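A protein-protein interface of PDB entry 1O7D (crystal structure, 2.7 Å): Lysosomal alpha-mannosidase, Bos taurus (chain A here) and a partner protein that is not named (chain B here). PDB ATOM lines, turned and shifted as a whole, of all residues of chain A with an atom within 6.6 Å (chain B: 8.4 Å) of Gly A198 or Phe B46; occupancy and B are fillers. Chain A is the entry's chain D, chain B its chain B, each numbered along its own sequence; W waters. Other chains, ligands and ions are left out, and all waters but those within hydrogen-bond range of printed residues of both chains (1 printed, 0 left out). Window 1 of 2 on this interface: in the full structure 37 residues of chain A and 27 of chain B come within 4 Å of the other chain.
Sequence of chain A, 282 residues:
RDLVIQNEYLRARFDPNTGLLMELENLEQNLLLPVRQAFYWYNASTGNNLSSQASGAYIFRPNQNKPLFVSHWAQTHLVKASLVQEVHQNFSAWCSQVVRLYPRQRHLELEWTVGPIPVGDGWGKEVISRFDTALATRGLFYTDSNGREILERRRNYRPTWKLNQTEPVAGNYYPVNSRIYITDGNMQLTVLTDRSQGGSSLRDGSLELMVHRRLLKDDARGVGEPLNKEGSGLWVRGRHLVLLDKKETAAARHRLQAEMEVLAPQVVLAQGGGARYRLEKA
N of Gly B44 is in hydrogen-bond range of O of Tyr A58 (2.9 Å).
The backbone carbonyl oxygen (O) of Gly B44 is in hydrogen-bond range of the guanidinium group (NH1) of Arg A213.
The backbone NH (N) of Tyr B45 is in hydrogen-bond range of the backbone carbonyl oxygen (O) of Tyr A58 (3.2 Å).
N of Gly A198 sits at hydrogen-bond distance from OG of Ser B47 (2.8 Å).
The side-chain hydroxyl of Ser B47 sits at hydrogen-bond distance from the backbone carbonyl oxygen of Met A210 (3.1 Å).
The side-chain hydroxyl (OG) of Ser B48 is in hydrogen-bond range of the backbone carbonyl oxygen (O) of Ala A57 (2.9 Å).
The side-chain hydroxyl of Ser B48 is in hydrogen-bond range of the guanidinium group of Arg A213 (3.2 Å).
O of Ser A196 sits close to O of Phe B46 (3.4 Å).
O of Tyr B34 lies within hydrogen-bond range of N of Trp B42 (3.0 Å).
The side-chain amino group (NZ) of Lys B53 sits at hydrogen-bond distance from the backbone carbonyl oxygen (O) of Tyr B45, 2.9 Å away.
The side-chain amino group (NZ) of Lys B53 sits at hydrogen-bond distance from the backbone carbonyl oxygen (O) of Ser B48.
The side-chain hydroxyl (OH) of Tyr A173 sits at hydrogen-bond distance from the side-chain carboxylate (OE2) of Glu A208 (2.5 Å).
The backbone NH (N) of Tyr A174 sits at hydrogen-bond distance from the backbone carbonyl oxygen (O) of Gly A199.
O of Gly A198 sits at hydrogen-bond distance from N of Met A210, 2.9 Å away.
Among the printed residues, pairs that only touch across the chains: Ala A57 with Tyr B45, Tyr A58 with Phe B41, Tyr A58 with Trp B42, Tyr A58 with Thr B43, Tyr A173 with Pro B33, Tyr A173 with Thr B43, Tyr A173 with Phe B46, Tyr A174 with Phe B32, Tyr A174 with Pro B33, Tyr A174 with Phe B46, Pro A175 with Phe B32, Pro A175 with Phe B46, Ser A196 with Lys B53, Gln A197 with Phe B46, Gln A197 with Ser B47, Gly A198 with Phe B46 and Val A211 with Pro B50.
Gly A198 touches two residues of chain B.
Of chain A, only Tyr A173 (3.8 Å), Tyr A174 (3.9 Å), Pro A175 (3.4 Å), Ser A196 (3.4 Å), Gln A197 (3.3 Å) and Gly A198 (3.7 Å) come within 4 Å of Phe B46.
No residue of chain B comes within 4 Å of Gly A199.
Of the printed residues of chain A, Trp B42 touches Tyr A58.
Of the printed residues of chain B, Arg A213 touches Gly B44 (3.2 Å) and Ser B48 (3.2 Å).
Printed residues of chain B within 4 Å of Pro A175: Phe B32 and Phe B46.
Printed residues of chain B within 4 Å of Gln A197: Phe B46 (3.3 Å) and Ser B47 (3.5 Å).
Tyr B34 touches none of the printed residues of chain A.
The nearest residue of chain A that does not touch Phe B46 is Gly A199 (5.5 Å).
Hydrophobic or aromatic side chains of chain B that line the printed part of chain A: Phe B32, Pro B33, Trp B42, Tyr B45, Phe B46 and Pro B50.
Among the printed residues, 25 pairs touch across the chains.
Water W1 lies within hydrogen-bond range of N of Arg B49 (2.8 Å) and O of Arg A213 (3.3 Å).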
ATOM      1  N   ALA A  57       1.674   3.595  14.704  1.00  0.00           N
ATOM      2  CA  ALA A  57       1.311   2.216  14.965  1.00  0.00           C
ATOM      3  C   ALA A  57      -0.188   1.944  14.719  1.00  0.00           C
ATOM      4  O   ALA A  57      -0.552   0.906  14.169  1.00  0.00           O
ATOM      5  CB  ALA A  57       1.694   1.859  16.384  1.00  0.00           C
ATOM      6  N   TYR A  58      -1.058   2.874  15.099  1.00  0.00           N
ATOM      7  CA  TYR A  58      -2.495   2.677  14.898  1.00  0.00           C
ATOM      8  C   TYR A  58      -3.051   3.323  13.643  1.00  0.00           C
ATOM      9  O   TYR A  58      -3.680   2.675  12.798  1.00  0.00           O
ATOM     10  CB  TYR A  58      -3.296   3.289  16.028  1.00  0.00           C
ATOM     11  CG  TYR A  58      -2.852   2.927  17.392  1.00  0.00           C
ATOM     12  CD1 TYR A  58      -3.372   1.823  18.043  1.00  0.00           C
ATOM     13  CD2 TYR A  58      -1.940   3.714  18.056  1.00  0.00           C
ATOM     14  CE1 TYR A  58      -2.998   1.520  19.327  1.00  0.00           C
ATOM     15  CE2 TYR A  58      -1.558   3.424  19.341  1.00  0.00           C
ATOM     16  CZ  TYR A  58      -2.088   2.327  19.973  1.00  0.00           C
ATOM     17  OH  TYR A  58      -1.700   2.043  21.257  1.00  0.00           O
ATOM     18  N   TYR A 173      -9.816   2.277   3.609  1.00  0.00           N
ATOM     19  CA  TYR A 173      -9.032   1.056   3.822  1.00  0.00           C
ATOM     20  C   TYR A 173      -9.758   0.089   4.758  1.00  0.00           C
ATOM     21  O   TYR A 173     -10.237   0.493   5.811  1.00  0.00           O
ATOM     22  CB  TYR A 173      -7.658   1.396   4.424  1.00  0.00           C
ATOM     23  CG  TYR A 173      -6.489   1.218   3.474  1.00  0.00           C
ATOM     24  CD1 TYR A 173      -6.003   2.279   2.722  1.00  0.00           C
ATOM     25  CD2 TYR A 173      -5.899  -0.017   3.293  1.00  0.00           C
ATOM     26  CE1 TYR A 173      -4.961   2.105   1.815  1.00  0.00           C
ATOM     27  CE2 TYR A 173      -4.864  -0.189   2.385  1.00  0.00           C
ATOM     28  CZ  TYR A 173      -4.404   0.867   1.655  1.00  0.00           C
ATOM     29  OH  TYR A 173      -3.392   0.667   0.749  1.00  0.00           O
ATOM     30  N   TYR A 174      -9.823  -1.186   4.395  1.00  0.00           N
ATOM     31  CA  TYR A 174     -10.506  -2.162   5.239  1.00  0.00           C
ATOM     32  C   TYR A 174      -9.634  -3.365   5.520  1.00  0.00           C
ATOM     33  O   TYR A 174      -8.735  -3.689   4.744  1.00  0.00           O
ATOM     34  CB  TYR A 174     -11.794  -2.633   4.574  1.00  0.00           C
ATOM     35  CG  TYR A 174     -12.809  -1.531   4.351  1.00  0.00           C
ATOM     36  CD1 TYR A 174     -12.634  -0.570   3.350  1.00  0.00           C
ATOM     37  CD2 TYR A 174     -13.942  -1.449   5.151  1.00  0.00           C
ATOM     38  CE1 TYR A 174     -13.563   0.436   3.159  1.00  0.00           C
ATOM     39  CE2 TYR A 174     -14.875  -0.446   4.971  1.00  0.00           C
ATOM     40  CZ  TYR A 174     -14.691   0.496   3.981  1.00  0.00           C
ATOM     41  OH  TYR A 174     -15.647   1.489   3.853  1.00  0.00           O
ATOM     42  N   PRO A 175      -9.887  -4.061   6.636  1.00  0.00           N
ATOM     43  CA  PRO A 175      -9.041  -5.222   6.904  1.00  0.00           C
ATOM     44  C   PRO A 175      -9.308  -6.400   5.981  1.00  0.00           C
ATOM     45  O   PRO A 175     -10.452  -6.789   5.756  1.00  0.00           O
ATOM     46  CB  PRO A 175      -9.341  -5.536   8.370  1.00  0.00           C
ATOM     47  CG  PRO A 175     -10.743  -5.083   8.531  1.00  0.00           C
ATOM     48  CD  PRO A 175     -10.777  -3.783   7.774  1.00  0.00           C
ATOM     49  N   VAL A 176      -8.238  -6.944   5.420  1.00  0.00           N
ATOM     50  CA  VAL A 176      -8.336  -8.106   4.552  1.00  0.00           C
ATOM     51  C   VAL A 176      -7.458  -9.181   5.194  1.00  0.00           C
ATOM     52  O   VAL A 176      -6.223  -9.073   5.209  1.00  0.00           O
ATOM     53  CB  VAL A 176      -7.859  -7.772   3.122  1.00  0.00           C
ATOM     54  CG1 VAL A 176      -6.800  -6.692   3.173  1.00  0.00           C
ATOM     55  CG2 VAL A 176      -7.336  -9.021   2.436  1.00  0.00           C
ATOM     56  N   ASN A 177      -8.106 -10.204   5.743  1.00  0.00           N
ATOM     57  CA  ASN A 177      -7.398 -11.281   6.415  1.00  0.00           C
ATOM     58  C   ASN A 177      -7.020 -12.462   5.545  1.00  0.00           C
ATOM     59  O   ASN A 177      -6.107 -13.220   5.900  1.00  0.00           O
ATOM     60  CB  ASN A 177      -8.216 -11.811   7.599  1.00  0.00           C
ATOM     61  CG  ASN A 177      -8.520 -10.742   8.621  1.00  0.00           C
ATOM     62  OD1 ASN A 177      -7.781  -9.773   8.769  1.00  0.00           O
ATOM     63  ND2 ASN A 177      -9.604 -10.918   9.344  1.00  0.00           N
ATOM     64  N   ILE A 180      -9.436 -10.499  -1.098  1.00  0.00           N
ATOM     65  CA  ILE A 180     -10.039  -9.265  -1.557  1.00  0.00           C
ATOM     66  C   ILE A 180     -10.234  -9.462  -3.060  1.00  0.00           C
ATOM     67  O   ILE A 180      -9.481 -10.212  -3.684  1.00  0.00           O
ATOM     68  CB  ILE A 180      -9.092  -8.065  -1.302  1.00  0.00           C
ATOM     69  CG1 ILE A 180      -9.747  -6.766  -1.784  1.00  0.00           C
ATOM     70  CG2 ILE A 180      -7.757  -8.303  -1.991  1.00  0.00           C
ATOM     71  CD1 ILE A 180      -8.899  -5.514  -1.561  1.00  0.00           C
ATOM     72  N   SER A 196      -2.810 -11.190   7.585  1.00  0.00           N
ATOM     73  CA  SER A 196      -3.787 -10.113   7.472  1.00  0.00           C
ATOM     74  C   SER A 196      -3.109  -8.819   7.039  1.00  0.00           C
ATOM     75  O   SER A 196      -2.018  -8.499   7.505  1.00  0.00           O
ATOM     76  CB  SER A 196      -4.544  -9.922   8.799  1.00  0.00           C
ATOM     77  OG  SER A 196      -3.676  -9.698   9.891  1.00  0.00           O
ATOM     78  N   GLN A 197      -3.743  -8.092   6.122  1.00  0.00           N
ATOM     79  CA  GLN A 197      -3.186  -6.827   5.633  1.00  0.00           C
ATOM     80  C   GLN A 197      -4.295  -5.776   5.453  1.00  0.00           C
ATOM     81  O   GLN A 197      -5.472  -6.055   5.664  1.00  0.00           O
ATOM     82  CB  GLN A 197      -2.459  -7.036   4.292  1.00  0.00           C
ATOM     83  CG  GLN A 197      -1.418  -8.158   4.275  1.00  0.00           C
ATOM     84  CD  GLN A 197      -0.616  -8.241   2.965  1.00  0.00           C
ATOM     85  OE1 GLN A 197      -1.166  -8.312   1.863  1.00  0.00           O
ATOM     86  NE2 GLN A 197       0.700  -8.246   3.099  1.00  0.00           N
ATOM     87  N   GLY A 198      -3.915  -4.562   5.074  1.00  0.00           N
ATOM     88  CA  GLY A 198      -4.897  -3.521   4.838  1.00  0.00           C
ATOM     89  C   GLY A 198      -5.088  -3.432   3.340  1.00  0.00           C
ATOM     90  O   GLY A 198      -4.222  -3.867   2.601  1.00  0.00           O
ATOM     91  N   GLY A 199      -6.216  -2.900   2.884  1.00  0.00           N
ATOM     92  CA  GLY A 199      -6.438  -2.782   1.454  1.00  0.00           C
ATOM     93  C   GLY A 199      -7.708  -2.037   1.064  1.00  0.00           C
ATOM     94  O   GLY A 199      -8.546  -1.732   1.922  1.00  0.00           O
ATOM     95  N   SER A 200      -7.843  -1.750  -0.234  1.00  0.00           N
ATOM     96  CA  SER A 200      -9.016  -1.062  -0.781  1.00  0.00           C
ATOM     97  C   SER A 200      -8.890  -0.791  -2.279  1.00  0.00           C
ATOM     98  O   SER A 200      -7.810  -0.952  -2.854  1.00  0.00           O
ATOM     99  CB  SER A 200      -9.233   0.270  -0.075  1.00  0.00           C
ATOM    100  OG  SER A 200     -10.405   0.896  -0.562  1.00  0.00           O
ATOM    101  N   GLU A 208      -5.360  -2.893  -4.082  1.00  0.00           N
ATOM    102  CA  GLU A 208      -4.108  -2.702  -3.354  1.00  0.00           C
ATOM    103  C   GLU A 208      -4.131  -3.201  -1.917  1.00  0.00           C
ATOM    104  O   GLU A 208      -5.103  -3.043  -1.190  1.00  0.00           O
ATOM    105  CB  GLU A 208      -3.675  -1.225  -3.365  1.00  0.00           C
ATOM    106  CG  GLU A 208      -4.622  -0.273  -2.637  1.00  0.00           C
ATOM    107  CD  GLU A 208      -4.115   1.164  -2.605  1.00  0.00           C
ATOM    108  OE1 GLU A 208      -3.989   1.788  -3.688  1.00  0.00           O
ATOM    109  OE2 GLU A 208      -3.845   1.668  -1.492  1.00  0.00           O
ATOM    110  N   LEU A 209      -3.024  -3.812  -1.524  1.00  0.00           N
ATOM    111  CA  LEU A 209      -2.840  -4.345  -0.186  1.00  0.00           C
ATOM    112  C   LEU A 209      -1.597  -3.674   0.400  1.00  0.00           C
ATOM    113  O   LEU A 209      -0.719  -3.234  -0.331  1.00  0.00           O
ATOM    114  CB  LEU A 209      -2.648  -5.855  -0.262  1.00  0.00           C
ATOM    115  CG  LEU A 209      -3.892  -6.599  -0.745  1.00  0.00           C
ATOM    116  CD1 LEU A 209      -3.501  -7.950  -1.298  1.00  0.00           C
ATOM    117  CD2 LEU A 209      -4.885  -6.735   0.409  1.00  0.00           C
ATOM    118  N   MET A 210      -1.518  -3.592   1.721  1.00  0.00           N
ATOM    119  CA  MET A 210      -0.377  -2.959   2.339  1.00  0.00           C
ATOM    120  C   MET A 210       0.623  -3.985   2.846  1.00  0.00           C
ATOM    121  O   MET A 210       0.379  -4.712   3.806  1.00  0.00           O
ATOM    122  CB  MET A 210      -0.830  -2.043   3.470  1.00  0.00           C
ATOM    123  CG  MET A 210       0.265  -1.109   3.950  1.00  0.00           C
ATOM    124  SD  MET A 210      -0.248   0.203   5.097  1.00  0.00           S
ATOM    125  CE  MET A 210      -0.894   1.452   3.918  1.00  0.00           C
ATOM    126  N   VAL A 211       1.767  -4.024   2.177  1.00  0.00           N
ATOM    127  CA  VAL A 211       2.841  -4.942   2.517  1.00  0.00           C
ATOM    128  C   VAL A 211       3.581  -4.617   3.818  1.00  0.00           C
ATOM    129  O   VAL A 211       3.744  -5.478   4.679  1.00  0.00           O
ATOM    130  CB  VAL A 211       3.892  -4.984   1.392  1.00  0.00           C
ATOM    131  CG1 VAL A 211       5.111  -5.699   1.877  1.00  0.00           C
ATOM    132  CG2 VAL A 211       3.338  -5.695   0.184  1.00  0.00           C
ATOM    133  N   ARG A 213       5.048  -1.039   6.563  1.00  0.00           N
ATOM    134  CA  ARG A 213       5.050   0.388   6.860  1.00  0.00           C
ATOM    135  C   ARG A 213       6.053   0.714   7.961  1.00  0.00           C
ATOM    136  O   ARG A 213       6.294  -0.089   8.859  1.00  0.00           O
ATOM    137  CB  ARG A 213       3.632   0.858   7.235  1.00  0.00           C
ATOM    138  CG  ARG A 213       2.989   0.163   8.420  1.00  0.00           C
ATOM    139  CD  ARG A 213       1.459   0.285   8.362  1.00  0.00           C
ATOM    140  NE  ARG A 213       0.977   1.669   8.356  1.00  0.00           N
ATOM    141  CZ  ARG A 213       0.664   2.378   9.446  1.00  0.00           C
ATOM    142  NH1 ARG A 213       0.768   1.849  10.659  1.00  0.00           N
ATOM    143  NH2 ARG A 213       0.252   3.634   9.326  1.00  0.00           N
ATOM    144  N   ASP B  30     -20.479  -4.510   8.988  1.00  0.00           N
ATOM    145  CA  ASP B  30     -19.397  -4.390   9.968  1.00  0.00           C
ATOM    146  C   ASP B  30     -19.242  -2.943  10.425  1.00  0.00           C
ATOM    147  O   ASP B  30     -19.908  -2.045   9.890  1.00  0.00           O
ATOM    148  CB  ASP B  30     -18.086  -4.854   9.326  1.00  0.00           C
ATOM    149  CG  ASP B  30     -17.726  -4.040   8.112  1.00  0.00           C
ATOM    150  OD1 ASP B  30     -18.561  -3.924   7.191  1.00  0.00           O
ATOM    151  OD2 ASP B  30     -16.612  -3.502   8.069  1.00  0.00           O
ATOM    152  N   PHE B  31     -18.397  -2.730  11.432  1.00  0.00           N
ATOM    153  CA  PHE B  31     -18.090  -1.403  11.943  1.00  0.00           C
ATOM    154  C   PHE B  31     -16.703  -0.884  11.514  1.00  0.00           C
ATOM    155  O   PHE B  31     -16.037  -0.275  12.333  1.00  0.00           O
ATOM    156  CB  PHE B  31     -18.105  -1.389  13.475  1.00  0.00           C
ATOM    157  CG  PHE B  31     -19.464  -1.552  14.032  1.00  0.00           C
ATOM    158  CD1 PHE B  31     -20.333  -0.465  14.146  1.00  0.00           C
ATOM    159  CD2 PHE B  31     -19.880  -2.786  14.471  1.00  0.00           C
ATOM    160  CE1 PHE B  31     -21.599  -0.622  14.729  1.00  0.00           C
ATOM    161  CE2 PHE B  31     -21.134  -2.962  15.053  1.00  0.00           C
ATOM    162  CZ  PHE B  31     -22.000  -1.880  15.190  1.00  0.00           C
ATOM    163  N   PHE B  32     -16.214  -1.170  10.316  1.00  0.00           N
ATOM    164  CA  PHE B  32     -14.966  -0.668   9.807  1.00  0.00           C
ATOM    165  C   PHE B  32     -15.359   0.363   8.829  1.00  0.00           C
ATOM    166  O   PHE B  32     -16.352   0.203   8.125  1.00  0.00           O
ATOM    167  CB  PHE B  32     -14.224  -1.788   9.157  1.00  0.00           C
ATOM    168  CG  PHE B  32     -13.632  -2.711  10.248  1.00  0.00           C
ATOM    169  CD1 PHE B  32     -12.560  -2.288  11.098  1.00  0.00           C
ATOM    170  CD2 PHE B  32     -14.148  -3.985  10.452  1.00  0.00           C
ATOM    171  CE1 PHE B  32     -12.055  -3.178  12.122  1.00  0.00           C
ATOM    172  CE2 PHE B  32     -13.666  -4.835  11.433  1.00  0.00           C
ATOM    173  CZ  PHE B  32     -12.619  -4.444  12.239  1.00  0.00           C
ATOM    174  N   PRO B  33     -14.580   1.455   8.706  1.00  0.00           N
ATOM    175  CA  PRO B  33     -13.350   1.792   9.443  1.00  0.00           C
ATOM    176  C   PRO B  33     -13.662   2.529  10.715  1.00  0.00           C
ATOM    177  O   PRO B  33     -14.632   3.288  10.798  1.00  0.00           O
ATOM    178  CB  PRO B  33     -12.580   2.669   8.446  1.00  0.00           C
ATOM    179  CG  PRO B  33     -13.146   2.308   7.144  1.00  0.00           C
ATOM    180  CD  PRO B  33     -14.608   2.148   7.394  1.00  0.00           C
ATOM    181  N   TYR B  34     -12.832   2.297  11.714  1.00  0.00           N
ATOM    182  CA  TYR B  34     -12.962   2.993  12.979  1.00  0.00           C
ATOM    183  C   TYR B  34     -12.237   4.350  12.894  1.00  0.00           C
ATOM    184  O   TYR B  34     -11.123   4.430  12.395  1.00  0.00           O
ATOM    185  CB  TYR B  34     -12.325   2.166  14.077  1.00  0.00           C
ATOM    186  CG  TYR B  34     -12.310   2.944  15.378  1.00  0.00           C
ATOM    187  CD1 TYR B  34     -13.449   3.607  15.892  1.00  0.00           C
ATOM    188  CD2 TYR B  34     -11.140   3.031  16.093  1.00  0.00           C
ATOM    189  CE1 TYR B  34     -13.370   4.331  17.125  1.00  0.00           C
ATOM    190  CE2 TYR B  34     -11.055   3.723  17.290  1.00  0.00           C
ATOM    191  CZ  TYR B  34     -12.188   4.380  17.790  1.00  0.00           C
ATOM    192  OH  TYR B  34     -12.173   5.102  18.942  1.00  0.00           O
ATOM    193  N   PHE B  41      -7.725   7.817  11.205  1.00  0.00           N
ATOM    194  CA  PHE B  41      -8.347   6.510  11.113  1.00  0.00           C
ATOM    195  C   PHE B  41      -7.462   5.443  11.703  1.00  0.00           C
ATOM    196  O   PHE B  41      -6.234   5.498  11.583  1.00  0.00           O
ATOM    197  CB  PHE B  41      -8.623   6.159   9.662  1.00  0.00           C
ATOM    198  CG  PHE B  41      -9.756   6.932   9.070  1.00  0.00           C
ATOM    199  CD1 PHE B  41     -11.074   6.489   9.209  1.00  0.00           C
ATOM    200  CD2 PHE B  41      -9.510   8.113   8.374  1.00  0.00           C
ATOM    201  CE1 PHE B  41     -12.135   7.214   8.664  1.00  0.00           C
ATOM    202  CE2 PHE B  41     -10.563   8.850   7.824  1.00  0.00           C
ATOM    203  CZ  PHE B  41     -11.880   8.395   7.969  1.00  0.00           C
ATOM    204  N   TRP B  42      -8.089   4.463  12.332  1.00  0.00           N
ATOM    205  CA  TRP B  42      -7.340   3.386  12.927  1.00  0.00           C
ATOM    206  C   TRP B  42      -7.246   2.276  11.896  1.00  0.00           C
ATOM    207  O   TRP B  42      -7.602   1.145  12.167  1.00  0.00           O
ATOM    208  CB  TRP B  42      -8.046   2.907  14.193  1.00  0.00           C
ATOM    209  CG  TRP B  42      -8.053   3.931  15.310  1.00  0.00           C
ATOM    210  CD1 TRP B  42      -8.431   5.257  15.239  1.00  0.00           C
ATOM    211  CD2 TRP B  42      -7.739   3.682  16.679  1.00  0.00           C
ATOM    212  NE1 TRP B  42      -8.375   5.832  16.489  1.00  0.00           N
ATOM    213  CE2 TRP B  42      -7.954   4.888  17.389  1.00  0.00           C
ATOM    214  CE3 TRP B  42      -7.298   2.553  17.379  1.00  0.00           C
ATOM    215  CZ2 TRP B  42      -7.741   4.986  18.770  1.00  0.00           C
ATOM    216  CZ3 TRP B  42      -7.088   2.653  18.748  1.00  0.00           C
ATOM    217  CH2 TRP B  42      -7.310   3.860  19.429  1.00  0.00           C
ATOM    218  N   THR B  43      -6.767   2.606  10.706  1.00  0.00           N
ATOM    219  CA  THR B  43      -6.641   1.607   9.664  1.00  0.00           C
ATOM    220  C   THR B  43      -5.193   1.214   9.364  1.00  0.00           C
ATOM    221  O   THR B  43      -4.931   0.406   8.475  1.00  0.00           O
ATOM    222  CB  THR B  43      -7.316   2.091   8.370  1.00  0.00           C
ATOM    223  OG1 THR B  43      -6.671   3.284   7.906  1.00  0.00           O
ATOM    224  CG2 THR B  43      -8.790   2.380   8.632  1.00  0.00           C
ATOM    225  N   GLY B  44      -4.258   1.766  10.126  1.00  0.00           N
ATOM    226  CA  GLY B  44      -2.856   1.463   9.899  1.00  0.00           C
ATOM    227  C   GLY B  44      -2.369   0.175  10.537  1.00  0.00           C
ATOM    228  O   GLY B  44      -1.390  -0.422  10.070  1.00  0.00           O
ATOM    229  N   TYR B  45      -3.041  -0.264  11.599  1.00  0.00           N
ATOM    230  CA  TYR B  45      -2.635  -1.489  12.272  1.00  0.00           C
ATOM    231  C   TYR B  45      -3.087  -2.720  11.498  1.00  0.00           C
ATOM    232  O   TYR B  45      -2.805  -3.852  11.899  1.00  0.00           O
ATOM    233  CB  TYR B  45      -3.189  -1.543  13.700  1.00  0.00           C
ATOM    234  CG  TYR B  45      -4.667  -1.862  13.817  1.00  0.00           C
ATOM    235  CD1 TYR B  45      -5.635  -0.887  13.593  1.00  0.00           C
ATOM    236  CD2 TYR B  45      -5.095  -3.143  14.170  1.00  0.00           C
ATOM    237  CE1 TYR B  45      -6.996  -1.176  13.717  1.00  0.00           C
ATOM    238  CE2 TYR B  45      -6.448  -3.442  14.295  1.00  0.00           C
ATOM    239  CZ  TYR B  45      -7.395  -2.451  14.065  1.00  0.00           C
ATOM    240  OH  TYR B  45      -8.740  -2.741  14.168  1.00  0.00           O
ATOM    241  N   PHE B  46      -3.797  -2.509  10.396  1.00  0.00           N
ATOM    242  CA  PHE B  46      -4.249  -3.630   9.597  1.00  0.00           C
ATOM    243  C   PHE B  46      -3.039  -4.305   8.988  1.00  0.00           C
ATOM    244  O   PHE B  46      -3.092  -5.469   8.608  1.00  0.00           O
ATOM    245  CB  PHE B  46      -5.197  -3.171   8.495  1.00  0.00           C
ATOM    246  CG  PHE B  46      -6.513  -2.646   9.005  1.00  0.00           C
ATOM    247  CD1 PHE B  46      -6.975  -2.994  10.270  1.00  0.00           C
ATOM    248  CD2 PHE B  46      -7.300  -1.819   8.206  1.00  0.00           C
ATOM    249  CE1 PHE B  46      -8.188  -2.528  10.731  1.00  0.00           C
ATOM    250  CE2 PHE B  46      -8.520  -1.347   8.662  1.00  0.00           C
ATOM    251  CZ  PHE B  46      -8.962  -1.704   9.925  1.00  0.00           C
ATOM    252  N   SER B  47      -1.934  -3.571   8.918  1.00  0.00           N
ATOM    253  CA  SER B  47      -0.712  -4.102   8.347  1.00  0.00           C
ATOM    254  C   SER B  47       0.477  -3.909   9.258  1.00  0.00           C
ATOM    255  O   SER B  47       1.545  -4.426   8.988  1.00  0.00           O
ATOM    256  CB  SER B  47      -0.438  -3.446   7.001  1.00  0.00           C
ATOM    257  OG  SER B  47      -1.466  -3.777   6.090  1.00  0.00           O
ATOM    258  N   SER B  48       0.310  -3.169  10.341  1.00  0.00           N
ATOM    259  CA  SER B  48       1.422  -2.955  11.248  1.00  0.00           C
ATOM    260  C   SER B  48       2.075  -4.275  11.673  1.00  0.00           C
ATOM    261  O   SER B  48       1.383  -5.254  11.984  1.00  0.00           O
ATOM    262  CB  SER B  48       0.942  -2.192  12.478  1.00  0.00           C
ATOM    263  OG  SER B  48       0.395  -0.948  12.102  1.00  0.00           O
ATOM    264  N   ARG B  49       3.409  -4.295  11.680  1.00  0.00           N
ATOM    265  CA  ARG B  49       4.186  -5.476  12.081  1.00  0.00           C
ATOM    266  C   ARG B  49       3.920  -6.746  11.250  1.00  0.00           C
ATOM    267  O   ARG B  49       3.457  -7.757  11.777  1.00  0.00           O
ATOM    268  CB  ARG B  49       3.938  -5.803  13.564  1.00  0.00           C
ATOM    269  CG  ARG B  49       4.425  -4.765  14.545  1.00  0.00           C
ATOM    270  CD  ARG B  49       4.387  -5.298  15.966  1.00  0.00           C
ATOM    271  NE  ARG B  49       4.806  -4.294  16.944  1.00  0.00           N
ATOM    272  CZ  ARG B  49       6.056  -3.856  17.098  1.00  0.00           C
ATOM    273  NH1 ARG B  49       7.035  -4.335  16.346  1.00  0.00           N
ATOM    274  NH2 ARG B  49       6.330  -2.924  18.001  1.00  0.00           N
ATOM    275  N   PRO B  50       4.241  -6.716   9.946  1.00  0.00           N
ATOM    276  CA  PRO B  50       4.049  -7.840   9.017  1.00  0.00           C
ATOM    277  C   PRO B  50       4.631  -9.165   9.510  1.00  0.00           C
ATOM    278  O   PRO B  50       3.977 -10.210   9.451  1.00  0.00           O
ATOM    279  CB  PRO B  50       4.750  -7.364   7.748  1.00  0.00           C
ATOM    280  CG  PRO B  50       4.626  -5.887   7.826  1.00  0.00           C
ATOM    281  CD  PRO B  50       4.914  -5.596   9.270  1.00  0.00           C
ATOM    282  N   LYS B  53       2.676 -10.666  12.425  1.00  0.00           N
ATOM    283  CA  LYS B  53       1.388 -11.066  11.890  1.00  0.00           C
ATOM    284  C   LYS B  53       1.489 -12.414  11.179  1.00  0.00           C
ATOM    285  O   LYS B  53       0.640 -13.276  11.367  1.00  0.00           O
ATOM    286  CB  LYS B  53       0.837  -9.982  10.958  1.00  0.00           C
ATOM    287  CG  LYS B  53      -0.017  -8.931  11.671  1.00  0.00           C
ATOM    288  CD  LYS B  53      -0.364  -7.742  10.762  1.00  0.00           C
ATOM    289  CE  LYS B  53      -1.458  -6.837  11.356  1.00  0.00           C
ATOM    290  NZ  LYS B  53      -1.038  -6.049  12.540  1.00  0.00           N
HETATM  291  O   HOH W   1       5.436  -2.683  10.632  1.00  0.00           O
